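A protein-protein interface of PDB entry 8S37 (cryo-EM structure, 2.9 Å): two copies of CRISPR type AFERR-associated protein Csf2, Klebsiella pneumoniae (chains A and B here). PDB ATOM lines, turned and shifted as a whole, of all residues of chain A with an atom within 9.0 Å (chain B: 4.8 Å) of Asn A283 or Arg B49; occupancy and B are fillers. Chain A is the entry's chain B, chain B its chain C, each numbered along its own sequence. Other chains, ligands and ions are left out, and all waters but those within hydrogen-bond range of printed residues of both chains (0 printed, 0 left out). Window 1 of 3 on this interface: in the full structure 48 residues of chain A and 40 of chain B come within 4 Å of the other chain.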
ATOM      1  N   THR A  17      14.391  -8.274   8.203  1.00  0.00           N
ATOM      2  CA  THR A  17      13.799  -7.190   8.976  1.00  0.00           C
ATOM      3  C   THR A  17      12.284  -7.218   8.845  1.00  0.00           C
ATOM      4  O   THR A  17      11.737  -7.720   7.864  1.00  0.00           O
ATOM      5  CB  THR A  17      14.315  -5.824   8.516  1.00  0.00           C
ATOM      6  OG1 THR A  17      13.681  -4.792   9.278  1.00  0.00           O
ATOM      7  CG2 THR A  17      14.030  -5.608   7.038  1.00  0.00           C
ATOM      8  N   GLY A 142      20.451  -0.527   7.883  1.00  0.00           N
ATOM      9  CA  GLY A 142      19.959   0.694   7.274  1.00  0.00           C
ATOM     10  C   GLY A 142      20.739   1.884   7.782  1.00  0.00           C
ATOM     11  O   GLY A 142      21.971   1.931   7.699  1.00  0.00           O
ATOM     12  N   ILE A 236      18.545   8.887   8.207  1.00  0.00           N
ATOM     13  CA  ILE A 236      17.600   7.782   8.125  1.00  0.00           C
ATOM     14  C   ILE A 236      17.708   6.972   9.407  1.00  0.00           C
ATOM     15  O   ILE A 236      18.801   6.545   9.793  1.00  0.00           O
ATOM     16  CB  ILE A 236      17.886   6.909   6.894  1.00  0.00           C
ATOM     17  CG1 ILE A 236      18.084   7.776   5.648  1.00  0.00           C
ATOM     18  CG2 ILE A 236      16.767   5.900   6.683  1.00  0.00           C
ATOM     19  CD1 ILE A 236      17.039   8.859   5.455  1.00  0.00           C
ATOM     20  N   TYR A 239      16.971   0.515  11.107  1.00  0.00           N
ATOM     21  CA  TYR A 239      15.999  -0.524  11.417  1.00  0.00           C
ATOM     22  C   TYR A 239      16.720  -1.739  11.974  1.00  0.00           C
ATOM     23  O   TYR A 239      17.799  -2.099  11.503  1.00  0.00           O
ATOM     24  CB  TYR A 239      15.179  -0.917  10.184  1.00  0.00           C
ATOM     25  CG  TYR A 239      15.993  -1.319   8.977  1.00  0.00           C
ATOM     26  CD1 TYR A 239      16.515  -2.598   8.858  1.00  0.00           C
ATOM     27  CD2 TYR A 239      16.219  -0.425   7.947  1.00  0.00           C
ATOM     28  CE1 TYR A 239      17.253  -2.965   7.757  1.00  0.00           C
ATOM     29  CE2 TYR A 239      16.945  -0.787   6.838  1.00  0.00           C
ATOM     30  CZ  TYR A 239      17.464  -2.055   6.748  1.00  0.00           C
ATOM     31  OH  TYR A 239      18.196  -2.412   5.641  1.00  0.00           O
ATOM     32  N   ARG A 277      12.253 -13.882  -0.356  1.00  0.00           N
ATOM     33  CA  ARG A 277      12.324 -12.617   0.362  1.00  0.00           C
ATOM     34  C   ARG A 277      11.279 -12.600   1.466  1.00  0.00           C
ATOM     35  O   ARG A 277      10.086 -12.783   1.199  1.00  0.00           O
ATOM     36  CB  ARG A 277      12.121 -11.439  -0.590  1.00  0.00           C
ATOM     37  CG  ARG A 277      12.581 -10.109  -0.014  1.00  0.00           C
ATOM     38  CD  ARG A 277      12.700  -9.029  -1.078  1.00  0.00           C
ATOM     39  NE  ARG A 277      13.655  -9.386  -2.119  1.00  0.00           N
ATOM     40  CZ  ARG A 277      14.973  -9.379  -1.970  1.00  0.00           C
ATOM     41  NH1 ARG A 277      15.540  -9.036  -0.824  1.00  0.00           N
ATOM     42  NH2 ARG A 277      15.743  -9.730  -2.994  1.00  0.00           N
ATOM     43  N   GLY A 279       9.939 -10.266   4.816  1.00  0.00           N
ATOM     44  CA  GLY A 279       9.997  -9.026   5.561  1.00  0.00           C
ATOM     45  C   GLY A 279       9.941  -7.805   4.671  1.00  0.00           C
ATOM     46  O   GLY A 279       9.354  -7.857   3.585  1.00  0.00           O
ATOM     47  N   GLY A 280      10.551  -6.707   5.115  1.00  0.00           N
ATOM     48  CA  GLY A 280      10.598  -5.494   4.321  1.00  0.00           C
ATOM     49  C   GLY A 280      11.995  -4.982   4.047  1.00  0.00           C
ATOM     50  O   GLY A 280      12.945  -5.763   3.952  1.00  0.00           O
ATOM     51  N   HIS A 281      12.119  -3.657   3.954  1.00  0.00           N
ATOM     52  CA  HIS A 281      13.337  -2.976   3.528  1.00  0.00           C
ATOM     53  C   HIS A 281      13.972  -3.680   2.336  1.00  0.00           C
ATOM     54  O   HIS A 281      15.194  -3.847   2.273  1.00  0.00           O
ATOM     55  CB  HIS A 281      14.301  -2.834   4.699  1.00  0.00           C
ATOM     56  CG  HIS A 281      13.827  -1.858   5.727  1.00  0.00           C
ATOM     57  ND1 HIS A 281      13.286  -2.247   6.934  1.00  0.00           N
ATOM     58  CD2 HIS A 281      13.768  -0.506   5.708  1.00  0.00           C
ATOM     59  CE1 HIS A 281      12.937  -1.175   7.624  1.00  0.00           C
ATOM     60  NE2 HIS A 281      13.222  -0.106   6.904  1.00  0.00           N
ATOM     61  N   ALA A 282      13.140  -4.076   1.374  1.00  0.00           N
ATOM     62  CA  ALA A 282      13.609  -4.771   0.186  1.00  0.00           C
ATOM     63  C   ALA A 282      14.397  -3.856  -0.735  1.00  0.00           C
ATOM     64  O   ALA A 282      15.082  -4.352  -1.633  1.00  0.00           O
ATOM     65  CB  ALA A 282      12.427  -5.373  -0.573  1.00  0.00           C
ATOM     66  N   ASN A 283      14.318  -2.541  -0.532  1.00  0.00           N
ATOM     67  CA  ASN A 283      15.176  -1.630  -1.276  1.00  0.00           C
ATOM     68  C   ASN A 283      16.639  -1.859  -0.929  1.00  0.00           C
ATOM     69  O   ASN A 283      17.521  -1.610  -1.757  1.00  0.00           O
ATOM     70  CB  ASN A 283      14.775  -0.181  -0.993  1.00  0.00           C
ATOM     71  CG  ASN A 283      14.756   0.145   0.488  1.00  0.00           C
ATOM     72  OD1 ASN A 283      15.304  -0.592   1.308  1.00  0.00           O
ATOM     73  ND2 ASN A 283      14.120   1.255   0.840  1.00  0.00           N
ATOM     74  N   HIS A 284      16.915  -2.329   0.286  1.00  0.00           N
ATOM     75  CA  HIS A 284      18.251  -2.743   0.689  1.00  0.00           C
ATOM     76  C   HIS A 284      18.441  -4.249   0.550  1.00  0.00           C
ATOM     77  O   HIS A 284      19.287  -4.828   1.239  1.00  0.00           O
ATOM     78  CB  HIS A 284      18.524  -2.308   2.127  1.00  0.00           C
ATOM     79  CG  HIS A 284      18.232  -0.864   2.382  1.00  0.00           C
ATOM     80  ND1 HIS A 284      17.895  -0.384   3.628  1.00  0.00           N
ATOM     81  CD2 HIS A 284      18.225   0.206   1.553  1.00  0.00           C
ATOM     82  CE1 HIS A 284      17.690   0.918   3.556  1.00  0.00           C
ATOM     83  NE2 HIS A 284      17.883   1.302   2.307  1.00  0.00           N
ATOM     84  N   ASN A 285      17.650  -4.893  -0.307  1.00  0.00           N
ATOM     85  CA  ASN A 285      17.700  -6.334  -0.542  1.00  0.00           C
ATOM     86  C   ASN A 285      17.487  -7.142   0.729  1.00  0.00           C
ATOM     87  O   ASN A 285      17.871  -8.313   0.792  1.00  0.00           O
ATOM     88  CB  ASN A 285      19.025  -6.748  -1.186  1.00  0.00           C
ATOM     89  CG  ASN A 285      18.927  -8.057  -1.942  1.00  0.00           C
ATOM     90  OD1 ASN A 285      17.837  -8.567  -2.194  1.00  0.00           O
ATOM     91  ND2 ASN A 285      20.074  -8.608  -2.310  1.00  0.00           N
ATOM     92  N   CYS A 286      16.881  -6.550   1.750  1.00  0.00           N
ATOM     93  CA  CYS A 286      16.615  -7.287   2.972  1.00  0.00           C
ATOM     94  C   CYS A 286      15.588  -8.376   2.708  1.00  0.00           C
ATOM     95  O   CYS A 286      14.673  -8.205   1.897  1.00  0.00           O
ATOM     96  CB  CYS A 286      16.110  -6.339   4.054  1.00  0.00           C
ATOM     97  SG  CYS A 286      17.345  -5.167   4.634  1.00  0.00           S
ATOM     98  N   GLY A 287      15.750  -9.506   3.389  1.00  0.00           N
ATOM     99  CA  GLY A 287      14.787 -10.584   3.360  1.00  0.00           C
ATOM    100  C   GLY A 287      15.252 -11.834   2.649  1.00  0.00           C
ATOM    101  O   GLY A 287      14.655 -12.898   2.858  1.00  0.00           O
ATOM    102  N   GLY B  45      24.470  -1.479   2.372  1.00  0.00           N
ATOM    103  CA  GLY B  45      23.766  -1.523   1.107  1.00  0.00           C
ATOM    104  C   GLY B  45      23.138  -0.198   0.737  1.00  0.00           C
ATOM    105  O   GLY B  45      22.839   0.029  -0.436  1.00  0.00           O
ATOM    106  N   THR B  46      22.949   0.693   1.713  1.00  0.00           N
ATOM    107  CA  THR B  46      22.396   2.007   1.414  1.00  0.00           C
ATOM    108  C   THR B  46      23.379   2.847   0.613  1.00  0.00           C
ATOM    109  O   THR B  46      22.984   3.544  -0.326  1.00  0.00           O
ATOM    110  CB  THR B  46      22.026   2.727   2.708  1.00  0.00           C
ATOM    111  OG1 THR B  46      23.095   2.595   3.653  1.00  0.00           O
ATOM    112  CG2 THR B  46      20.758   2.148   3.299  1.00  0.00           C
ATOM    113  N   SER B  47      24.663   2.793   0.966  1.00  0.00           N
ATOM    114  CA  SER B  47      25.660   3.540   0.208  1.00  0.00           C
ATOM    115  C   SER B  47      25.774   3.011  -1.214  1.00  0.00           C
ATOM    116  O   SER B  47      25.847   3.791  -2.172  1.00  0.00           O
ATOM    117  CB  SER B  47      27.009   3.476   0.919  1.00  0.00           C
ATOM    118  OG  SER B  47      27.000   4.272   2.091  1.00  0.00           O
ATOM    119  N   ILE B  48      25.781   1.686  -1.375  1.00  0.00           N
ATOM    120  CA  ILE B  48      25.847   1.110  -2.713  1.00  0.00           C
ATOM    121  C   ILE B  48      24.612   1.507  -3.505  1.00  0.00           C
ATOM    122  O   ILE B  48      24.697   1.882  -4.682  1.00  0.00           O
ATOM    123  CB  ILE B  48      25.989  -0.424  -2.645  1.00  0.00           C
ATOM    124  CG1 ILE B  48      27.180  -0.869  -1.783  1.00  0.00           C
ATOM    125  CG2 ILE B  48      26.152  -0.985  -4.042  1.00  0.00           C
ATOM    126  CD1 ILE B  48      28.529  -0.682  -2.440  1.00  0.00           C
ATOM    127  N   ARG B  49      23.444   1.446  -2.864  1.00  0.00           N
ATOM    128  CA  ARG B  49      22.201   1.786  -3.540  1.00  0.00           C
ATOM    129  C   ARG B  49      22.201   3.240  -3.974  1.00  0.00           C
ATOM    130  O   ARG B  49      21.788   3.559  -5.090  1.00  0.00           O
ATOM    131  CB  ARG B  49      21.014   1.510  -2.622  1.00  0.00           C
ATOM    132  CG  ARG B  49      19.686   1.434  -3.344  1.00  0.00           C
ATOM    133  CD  ARG B  49      18.575   1.054  -2.387  1.00  0.00           C
ATOM    134  NE  ARG B  49      17.471   0.356  -3.036  1.00  0.00           N
ATOM    135  CZ  ARG B  49      16.617   0.905  -3.890  1.00  0.00           C
ATOM    136  NH1 ARG B  49      16.770   2.143  -4.329  1.00  0.00           N
ATOM    137  NH2 ARG B  49      15.583   0.191  -4.319  1.00  0.00           N
ATOM    138  N   GLY B  50      22.671   4.136  -3.109  1.00  0.00           N
ATOM    139  CA  GLY B  50      22.708   5.541  -3.468  1.00  0.00           C
ATOM    140  C   GLY B  50      23.687   5.818  -4.591  1.00  0.00           C
ATOM    141  O   GLY B  50      23.391   6.586  -5.509  1.00  0.00           O
ATOM    142  N   THR B  51      24.868   5.201  -4.533  1.00  0.00           N
ATOM    143  CA  THR B  51      25.845   5.394  -5.597  1.00  0.00           C
ATOM    144  C   THR B  51      25.290   4.921  -6.932  1.00  0.00           C
ATOM    145  O   THR B  51      25.371   5.636  -7.939  1.00  0.00           O
ATOM    146  CB  THR B  51      27.139   4.656  -5.260  1.00  0.00           C
ATOM    147  OG1 THR B  51      27.713   5.211  -4.071  1.00  0.00           O
ATOM    148  CG2 THR B  51      28.133   4.776  -6.402  1.00  0.00           C
ATOM    149  N   LEU B  52      24.692   3.729  -6.960  1.00  0.00           N
ATOM    150  CA  LEU B  52      24.159   3.232  -8.222  1.00  0.00           C
ATOM    151  C   LEU B  52      22.924   4.008  -8.653  1.00  0.00           C
ATOM    152  O   LEU B  52      22.679   4.153  -9.852  1.00  0.00           O
ATOM    153  CB  LEU B  52      23.831   1.740  -8.127  1.00  0.00           C
ATOM    154  CG  LEU B  52      24.948   0.700  -8.316  1.00  0.00           C
ATOM    155  CD1 LEU B  52      25.804   0.957  -9.553  1.00  0.00           C
ATOM    156  CD2 LEU B  52      25.820   0.607  -7.087  1.00  0.00           C
ATOM    157  N   ARG B  53      22.154   4.546  -7.707  1.00  0.00           N
ATOM    158  CA  ARG B  53      20.996   5.346  -8.078  1.00  0.00           C
ATOM    159  C   ARG B  53      21.423   6.656  -8.715  1.00  0.00           C
ATOM    160  O   ARG B  53      20.827   7.096  -9.701  1.00  0.00           O
ATOM    161  CB  ARG B  53      20.112   5.604  -6.862  1.00  0.00           C
ATOM    162  CG  ARG B  53      18.835   6.339  -7.213  1.00  0.00           C
ATOM    163  CD  ARG B  53      17.796   6.240  -6.117  1.00  0.00           C
ATOM    164  NE  ARG B  53      16.534   6.843  -6.528  1.00  0.00           N
ATOM    165  CZ  ARG B  53      15.366   6.644  -5.931  1.00  0.00           C
ATOM    166  NH1 ARG B  53      15.248   5.839  -4.887  1.00  0.00           N
ATOM    167  NH2 ARG B  53      14.287   7.263  -6.398  1.00  0.00           N
ATOM    168  N   LEU B 115      12.839   1.005 -11.101  1.00  0.00           N
ATOM    169  CA  LEU B 115      14.022   0.383 -10.523  1.00  0.00           C
ATOM    170  C   LEU B 115      14.236   0.861  -9.091  1.00  0.00           C
ATOM    171  O   LEU B 115      14.175   0.072  -8.144  1.00  0.00           O
ATOM    172  CB  LEU B 115      15.232   0.703 -11.406  1.00  0.00           C
ATOM    173  CG  LEU B 115      16.424  -0.248 -11.433  1.00  0.00           C
ATOM    174  CD1 LEU B 115      16.006  -1.632 -11.891  1.00  0.00           C
ATOM    175  CD2 LEU B 115      17.494   0.306 -12.358  1.00  0.00           C
ATOM    176  N   PHE B 116      14.443   2.165  -8.916  1.00  0.00           N
ATOM    177  CA  PHE B 116      14.600   2.788  -7.605  1.00  0.00           C
ATOM    178  C   PHE B 116      13.295   3.496  -7.263  1.00  0.00           C
ATOM    179  O   PHE B 116      13.001   4.560  -7.816  1.00  0.00           O
ATOM    180  CB  PHE B 116      15.764   3.775  -7.598  1.00  0.00           C
ATOM    181  CG  PHE B 116      17.030   3.235  -8.197  1.00  0.00           C
ATOM    182  CD1 PHE B 116      17.273   3.353  -9.553  1.00  0.00           C
ATOM    183  CD2 PHE B 116      17.985   2.630  -7.403  1.00  0.00           C
ATOM    184  CE1 PHE B 116      18.437   2.864 -10.104  1.00  0.00           C
ATOM    185  CE2 PHE B 116      19.150   2.139  -7.951  1.00  0.00           C
ATOM    186  CZ  PHE B 116      19.377   2.257  -9.302  1.00  0.00           C
ATOM    187  N   GLY B 117      12.516   2.917  -6.358  1.00  0.00           N
ATOM    188  CA  GLY B 117      11.192   3.436  -6.104  1.00  0.00           C
ATOM    189  C   GLY B 117      11.222   4.817  -5.469  1.00  0.00           C
ATOM    190  O   GLY B 117      12.241   5.504  -5.405  1.00  0.00           O
ATOM    191  N   GLY B 123      10.370  -0.020  -4.818  1.00  0.00           N
ATOM    192  CA  GLY B 123      11.505  -0.102  -5.713  1.00  0.00           C
ATOM    193  C   GLY B 123      11.791  -1.523  -6.145  1.00  0.00           C
ATOM    194  O   GLY B 123      12.007  -2.397  -5.301  1.00  0.00           O
ATOM    195  N   VAL B 125      14.415  -2.641  -7.405  1.00  0.00           N
ATOM    196  CA  VAL B 125      15.814  -2.967  -7.159  1.00  0.00           C
ATOM    197  C   VAL B 125      16.070  -2.959  -5.658  1.00  0.00           C
ATOM    198  O   VAL B 125      15.745  -1.990  -4.964  1.00  0.00           O
ATOM    199  CB  VAL B 125      16.757  -2.007  -7.909  1.00  0.00           C
ATOM    200  CG1 VAL B 125      16.942  -0.688  -7.180  1.00  0.00           C
ATOM    201  CG2 VAL B 125      18.096  -2.672  -8.142  1.00  0.00           C
ATOM    202  N   GLY B 126      16.599  -4.067  -5.155  1.00  0.00           N
ATOM    203  CA  GLY B 126      17.083  -4.167  -3.798  1.00  0.00           C
ATOM    204  C   GLY B 126      18.576  -4.391  -3.802  1.00  0.00           C
ATOM    205  O   GLY B 126      19.053  -5.440  -4.244  1.00  0.00           O
ATOM    206  N   ILE B 127      19.321  -3.406  -3.321  1.00  0.00           N
ATOM    207  CA  ILE B 127      20.777  -3.426  -3.323  1.00  0.00           C
ATOM    208  C   ILE B 127      21.239  -3.844  -1.936  1.00  0.00           C
ATOM    209  O   ILE B 127      21.146  -3.064  -0.982  1.00  0.00           O
ATOM    210  CB  ILE B 127      21.348  -2.060  -3.715  1.00  0.00           C
ATOM    211  CG1 ILE B 127      20.736  -1.574  -5.036  1.00  0.00           C
ATOM    212  CG2 ILE B 127      22.845  -2.123  -3.815  1.00  0.00           C
ATOM    213  CD1 ILE B 127      20.886  -2.531  -6.197  1.00  0.00           C
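Asn A283 touches just these residues of chain B: Arg B49 (2.3 Å), Val B125 (3.7 Å), Gly B126 (3.3 Å) and Ile B127 (3.0 Å).
Of chain A, only Asn A283 comes within 4 Å of Arg B49.
Gly B126 touches just these residues of chain A: Ala A282 (3.0 Å), Asn A283 (3.3 Å) and Asn A285 (3.3 Å).
Printed residues of chain B within 4 Å of His A284: Thr B46 and Ile B127.
Printed residues of chain A within 4 Å of Ile B127: Asn A283 (3.0 Å), His A284 (3.3 Å) and Asn A285 (3.7 Å).
Printed residues of chain A within 4 Å of Val B125: Asn A283 (3.7 Å).
Of the printed residues of chain A, Thr B46 touches His A284 (3.2 Å).
Gly A142 touches none of the printed residues of chain B.
The nearest residue of chain A that does not touch Arg B49 is His A284 (4.05 Å).
The nearest printed residue of chain B that does not touch Ala A282 is Val B125 (4.1 Å).
The backbone carbonyl oxygen (O) of Asn A283 sits close to the guanidinium group (NE) of Arg B49, 2.3 Å away.
O of His A284 sits close to O of Ile B127, at 3.4 Å.
The backbone NH of Ile B127 lies within hydrogen-bond range of the backbone carbonyl oxygen of Asn A283, at 3.0 Å.
Among the printed residues, merely in contact across the chains: Ala A282 with Gly B126 (3.0 Å), His A284 with Thr B46 (3.2 Å), Asn A283 with Gly B126 (3.3 Å), Asn A285 with Gly B126 (3.3 Å), Asn A283 with Val B125 (3.7 Å) and Asn A285 with Ile B127 (3.7 Å).
Printed residues of chain A that touch a printed residue of chain B: Ala A282, Asn A283, His A284 and Asn A285.
Among the printed residues, 9 pairs touch across the chains.
Among the printed residues, no Asp or Glu carboxylate lies within 4 Å of a Lys or Arg side-chain nitrogen of the other chain.
The backbone carbonyl oxygen (O) of Leu B115 is in hydrogen-bond range of the backbone NH (N) of Val B125, 2.8 Å away.
A ring nitrogen (ND1) of His A284 lies within hydrogen-bond range of the side-chain hydroxyl (OH) of Tyr A239.
The backbone carbonyl oxygen of Val B125 sits close to the guanidinium group of Arg B49 (3.5 Å).
The guanidinium group (NH2) of Arg A277 is in hydrogen-bond range of the side-chain amide oxygen (OD1) of Asn A285 (2.5 Å).
A ring nitrogen (NE2) of His A284 lies close to the side-chain amide oxygen (OD1) of Asn A283 (3.4 Å).
O of His A281 sits close to OD1 of Asn A283 (3.4 Å).
No position is printed for both chains.
Of the 9 pairs that touch across the chains among the printed residues, none has its exchanged pair printed and touching as well.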
